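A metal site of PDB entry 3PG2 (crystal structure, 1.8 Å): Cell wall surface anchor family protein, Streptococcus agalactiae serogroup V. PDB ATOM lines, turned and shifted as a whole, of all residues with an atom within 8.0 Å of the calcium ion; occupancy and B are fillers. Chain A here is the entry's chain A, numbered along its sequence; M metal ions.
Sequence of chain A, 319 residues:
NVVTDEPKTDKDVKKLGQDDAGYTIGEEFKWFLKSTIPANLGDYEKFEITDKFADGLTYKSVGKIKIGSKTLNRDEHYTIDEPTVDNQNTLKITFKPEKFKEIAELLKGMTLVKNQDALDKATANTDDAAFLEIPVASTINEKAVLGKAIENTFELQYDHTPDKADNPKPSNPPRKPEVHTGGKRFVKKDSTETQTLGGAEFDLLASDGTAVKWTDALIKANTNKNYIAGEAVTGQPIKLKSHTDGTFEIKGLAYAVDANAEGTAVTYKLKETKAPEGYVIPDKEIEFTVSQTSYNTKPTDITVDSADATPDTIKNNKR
The calcium ion is bound by O of Ala 165.
OE1 of Glu 45 is bound to the calcium ion.
OD1 of Asp 159 is bound to the calcium ion, at 2.4 Å.
The calcium ion is bound by OG1 of Thr 161, 2.5 Å away.
The calcium ion is bound by OD1 of Asn 167 (2.5 Å).
The calcium ion is bound by OD1 of Asp 163 (2.5 Å).
O of Thr 161 binds the calcium ion (2.5 Å).
The calcium ion is bound by OD2 of Asp 159, at 2.6 Å.
The calcium ion has eight donor atoms within binding distance.
The backbone NH of Lys 164 lies within hydrogen-bond range of the side-chain carboxylate of Glu 45 (2.8 Å).
The backbone carbonyl oxygen (O) of Lys 46 is in hydrogen-bond range of the backbone NH (N) of Asp 159 (2.9 Å).
The nearest printed residue that does not touch the calcium ion is Asp 166 (4.6 Å).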
ATOM      1  N   ASP A  43     -21.364  16.840 -12.038  1.00  0.00           N
ATOM      2  CA  ASP A  43     -20.786  18.130 -11.612  1.00  0.00           C
ATOM      3  C   ASP A  43     -19.258  18.107 -11.440  1.00  0.00           C
ATOM      4  O   ASP A  43     -18.639  19.168 -11.338  1.00  0.00           O
ATOM      5  CB  ASP A  43     -21.372  18.564 -10.257  1.00  0.00           C
ATOM      6  CG  ASP A  43     -22.806  18.991 -10.350  1.00  0.00           C
ATOM      7  OD1 ASP A  43     -23.265  19.304 -11.467  1.00  0.00           O
ATOM      8  OD2 ASP A  43     -23.474  18.976  -9.289  1.00  0.00           O
ATOM      9  N   TYR A  44     -18.667  16.915 -11.385  1.00  0.00           N
ATOM     10  CA  TYR A  44     -17.291  16.799 -10.914  1.00  0.00           C
ATOM     11  C   TYR A  44     -16.269  17.410 -11.874  1.00  0.00           C
ATOM     12  O   TYR A  44     -16.364  17.229 -13.090  1.00  0.00           O
ATOM     13  CB  TYR A  44     -16.955  15.333 -10.593  1.00  0.00           C
ATOM     14  CG  TYR A  44     -17.404  14.919  -9.207  1.00  0.00           C
ATOM     15  CD1 TYR A  44     -18.709  15.151  -8.778  1.00  0.00           C
ATOM     16  CD2 TYR A  44     -16.519  14.278  -8.324  1.00  0.00           C
ATOM     17  CE1 TYR A  44     -19.144  14.768  -7.524  1.00  0.00           C
ATOM     18  CE2 TYR A  44     -16.958  13.886  -7.040  1.00  0.00           C
ATOM     19  CZ  TYR A  44     -18.268  14.129  -6.656  1.00  0.00           C
ATOM     20  OH  TYR A  44     -18.715  13.761  -5.405  1.00  0.00           O
ATOM     21  N   GLU A  45     -15.290  18.100 -11.303  1.00  0.00           N
ATOM     22  CA  GLU A  45     -14.228  18.750 -12.051  1.00  0.00           C
ATOM     23  C   GLU A  45     -12.914  17.971 -11.968  1.00  0.00           C
ATOM     24  O   GLU A  45     -11.956  18.299 -12.663  1.00  0.00           O
ATOM     25  CB  GLU A  45     -14.031  20.179 -11.527  1.00  0.00           C
ATOM     26  CG  GLU A  45     -15.266  21.072 -11.796  1.00  0.00           C
ATOM     27  CD  GLU A  45     -15.088  22.490 -11.302  1.00  0.00           C
ATOM     28  OE1 GLU A  45     -14.282  22.727 -10.382  1.00  0.00           O
ATOM     29  OE2 GLU A  45     -15.805  23.366 -11.809  1.00  0.00           O
ATOM     30  N   LYS A  46     -12.874  16.956 -11.126  1.00  0.00           N
ATOM     31  CA  LYS A  46     -11.688  16.108 -11.035  1.00  0.00           C
ATOM     32  C   LYS A  46     -12.087  14.798 -10.410  1.00  0.00           C
ATOM     33  O   LYS A  46     -12.894  14.775  -9.481  1.00  0.00           O
ATOM     34  CB  LYS A  46     -10.644  16.783 -10.127  1.00  0.00           C
ATOM     35  CG  LYS A  46      -9.232  16.177 -10.175  1.00  0.00           C
ATOM     36  CD  LYS A  46      -8.313  16.965  -9.243  1.00  0.00           C
ATOM     37  CE  LYS A  46      -7.042  16.205  -8.950  1.00  0.00           C
ATOM     38  NZ  LYS A  46      -6.021  16.407 -10.018  1.00  0.00           N
ATOM     39  N   TYR A 158     -10.896  13.944  -5.584  1.00  0.00           N
ATOM     40  CA  TYR A 158     -12.136  14.291  -6.296  1.00  0.00           C
ATOM     41  C   TYR A 158     -12.518  15.741  -6.076  1.00  0.00           C
ATOM     42  O   TYR A 158     -12.330  16.270  -4.979  1.00  0.00           O
ATOM     43  CB  TYR A 158     -13.282  13.377  -5.850  1.00  0.00           C
ATOM     44  CG  TYR A 158     -13.716  13.575  -4.411  1.00  0.00           C
ATOM     45  CD1 TYR A 158     -14.734  14.487  -4.107  1.00  0.00           C
ATOM     46  CD2 TYR A 158     -13.121  12.861  -3.358  1.00  0.00           C
ATOM     47  CE1 TYR A 158     -15.150  14.682  -2.790  1.00  0.00           C
ATOM     48  CE2 TYR A 158     -13.538  13.055  -2.041  1.00  0.00           C
ATOM     49  CZ  TYR A 158     -14.558  13.970  -1.770  1.00  0.00           C
ATOM     50  OH  TYR A 158     -14.996  14.175  -0.493  1.00  0.00           O
ATOM     51  N   ASP A 159     -13.044  16.382  -7.118  1.00  0.00           N
ATOM     52  CA  ASP A 159     -13.564  17.750  -7.002  1.00  0.00           C
ATOM     53  C   ASP A 159     -15.047  17.723  -7.354  1.00  0.00           C
ATOM     54  O   ASP A 159     -15.405  17.635  -8.527  1.00  0.00           O
ATOM     55  CB  ASP A 159     -12.762  18.667  -7.929  1.00  0.00           C
ATOM     56  CG  ASP A 159     -13.216  20.122  -7.855  1.00  0.00           C
ATOM     57  OD1 ASP A 159     -14.370  20.389  -7.439  1.00  0.00           O
ATOM     58  OD2 ASP A 159     -12.407  20.993  -8.222  1.00  0.00           O
ATOM     59  N   HIS A 160     -15.906  17.772  -6.342  1.00  0.00           N
ATOM     60  CA  HIS A 160     -17.366  17.694  -6.506  1.00  0.00           C
ATOM     61  C   HIS A 160     -18.046  19.047  -6.778  1.00  0.00           C
ATOM     62  O   HIS A 160     -19.229  19.082  -7.072  1.00  0.00           O
ATOM     63  CB  HIS A 160     -18.047  17.042  -5.295  1.00  0.00           C
ATOM     64  CG  HIS A 160     -18.038  17.889  -4.051  1.00  0.00           C
ATOM     65  ND1 HIS A 160     -19.138  18.614  -3.621  1.00  0.00           N
ATOM     66  CD2 HIS A 160     -17.072  18.103  -3.134  1.00  0.00           C
ATOM     67  CE1 HIS A 160     -18.843  19.232  -2.496  1.00  0.00           C
ATOM     68  NE2 HIS A 160     -17.598  18.946  -2.176  1.00  0.00           N
ATOM     69  N   THR A 161     -17.306  20.134  -6.670  1.00  0.00           N
ATOM     70  CA  THR A 161     -17.908  21.454  -6.817  1.00  0.00           C
ATOM     71  C   THR A 161     -17.782  21.977  -8.257  1.00  0.00           C
ATOM     72  O   THR A 161     -16.661  22.170  -8.726  1.00  0.00           O
ATOM     73  CB  THR A 161     -17.275  22.460  -5.808  1.00  0.00           C
ATOM     74  OG1 THR A 161     -15.852  22.527  -6.016  1.00  0.00           O
ATOM     75  CG2 THR A 161     -17.559  22.020  -4.402  1.00  0.00           C
ATOM     76  N   PRO A 162     -18.925  22.195  -8.962  1.00  0.00           N
ATOM     77  CA  PRO A 162     -18.857  22.755 -10.326  1.00  0.00           C
ATOM     78  C   PRO A 162     -18.720  24.292 -10.314  1.00  0.00           C
ATOM     79  O   PRO A 162     -19.526  25.022 -10.922  1.00  0.00           O
ATOM     80  CB  PRO A 162     -20.194  22.323 -10.943  1.00  0.00           C
ATOM     81  CG  PRO A 162     -21.155  22.256  -9.722  1.00  0.00           C
ATOM     82  CD  PRO A 162     -20.309  21.910  -8.530  1.00  0.00           C
ATOM     83  N   ASP A 163     -17.688  24.773  -9.631  1.00  0.00           N
ATOM     84  CA  ASP A 163     -17.521  26.197  -9.378  1.00  0.00           C
ATOM     85  C   ASP A 163     -16.333  26.823 -10.121  1.00  0.00           C
ATOM     86  O   ASP A 163     -16.004  27.991  -9.889  1.00  0.00           O
ATOM     87  CB  ASP A 163     -17.356  26.437  -7.871  1.00  0.00           C
ATOM     88  CG  ASP A 163     -16.169  25.688  -7.265  1.00  0.00           C
ATOM     89  OD1 ASP A 163     -15.452  24.988  -8.017  1.00  0.00           O
ATOM     90  OD2 ASP A 163     -15.960  25.795  -6.042  1.00  0.00           O
ATOM     91  N   LYS A 164     -15.666  26.048 -10.985  1.00  0.00           N
ATOM     92  CA  LYS A 164     -14.532  26.545 -11.780  1.00  0.00           C
ATOM     93  C   LYS A 164     -13.310  26.851 -10.906  1.00  0.00           C
ATOM     94  O   LYS A 164     -12.411  27.597 -11.322  1.00  0.00           O
ATOM     95  CB  LYS A 164     -14.931  27.786 -12.629  1.00  0.00           C
ATOM     96  CG  LYS A 164     -15.665  27.466 -13.936  1.00  0.00           C
ATOM     97  CD  LYS A 164     -16.965  26.733 -13.678  1.00  0.00           C
ATOM     98  CE  LYS A 164     -17.607  26.190 -14.956  1.00  0.00           C
ATOM     99  NZ  LYS A 164     -18.886  25.537 -14.564  1.00  0.00           N
ATOM    100  N   ALA A 165     -13.288  26.268  -9.713  1.00  0.00           N
ATOM    101  CA  ALA A 165     -12.147  26.389  -8.810  1.00  0.00           C
ATOM    102  C   ALA A 165     -11.606  24.984  -8.575  1.00  0.00           C
ATOM    103  O   ALA A 165     -12.365  24.045  -8.324  1.00  0.00           O
ATOM    104  CB  ALA A 165     -12.568  27.038  -7.502  1.00  0.00           C
ATOM    105  N   ASP A 166     -10.280  24.854  -8.697  1.00  0.00           N
ATOM    106  CA  ASP A 166      -9.590  23.583  -8.555  1.00  0.00           C
ATOM    107  C   ASP A 166      -9.374  23.264  -7.071  1.00  0.00           C
ATOM    108  O   ASP A 166      -8.315  23.515  -6.524  1.00  0.00           O
ATOM    109  CB  ASP A 166      -8.245  23.654  -9.300  1.00  0.00           C
ATOM    110  CG  ASP A 166      -7.529  22.302  -9.391  1.00  0.00           C
ATOM    111  OD1 ASP A 166      -8.104  21.244  -9.022  1.00  0.00           O
ATOM    112  OD2 ASP A 166      -6.366  22.308  -9.836  1.00  0.00           O
ATOM    113  N   ASN A 167     -10.397  22.681  -6.453  1.00  0.00           N
ATOM    114  CA  ASN A 167     -10.385  22.432  -5.002  1.00  0.00           C
ATOM    115  C   ASN A 167     -10.767  20.987  -4.629  1.00  0.00           C
ATOM    116  O   ASN A 167     -11.779  20.782  -3.956  1.00  0.00           O
ATOM    117  CB  ASN A 167     -11.286  23.450  -4.287  1.00  0.00           C
ATOM    118  CG  ASN A 167     -12.635  23.663  -4.988  1.00  0.00           C
ATOM    119  OD1 ASN A 167     -13.052  22.893  -5.881  1.00  0.00           O
ATOM    120  ND2 ASN A 167     -13.344  24.740  -4.581  1.00  0.00           N
ATOM    121  N   PRO A 168      -9.973  19.990  -5.071  1.00  0.00           N
ATOM    122  CA  PRO A 168     -10.299  18.578  -4.760  1.00  0.00           C
ATOM    123  C   PRO A 168     -10.103  18.225  -3.287  1.00  0.00           C
ATOM    124  O   PRO A 168      -9.418  18.941  -2.561  1.00  0.00           O
ATOM    125  CB  PRO A 168      -9.293  17.796  -5.598  1.00  0.00           C
ATOM    126  CG  PRO A 168      -8.065  18.722  -5.611  1.00  0.00           C
ATOM    127  CD  PRO A 168      -8.688  20.095  -5.794  1.00  0.00           C
HETATM  128 CA    CA M   1     -14.363  22.753  -7.964  1.00  0.00          CA
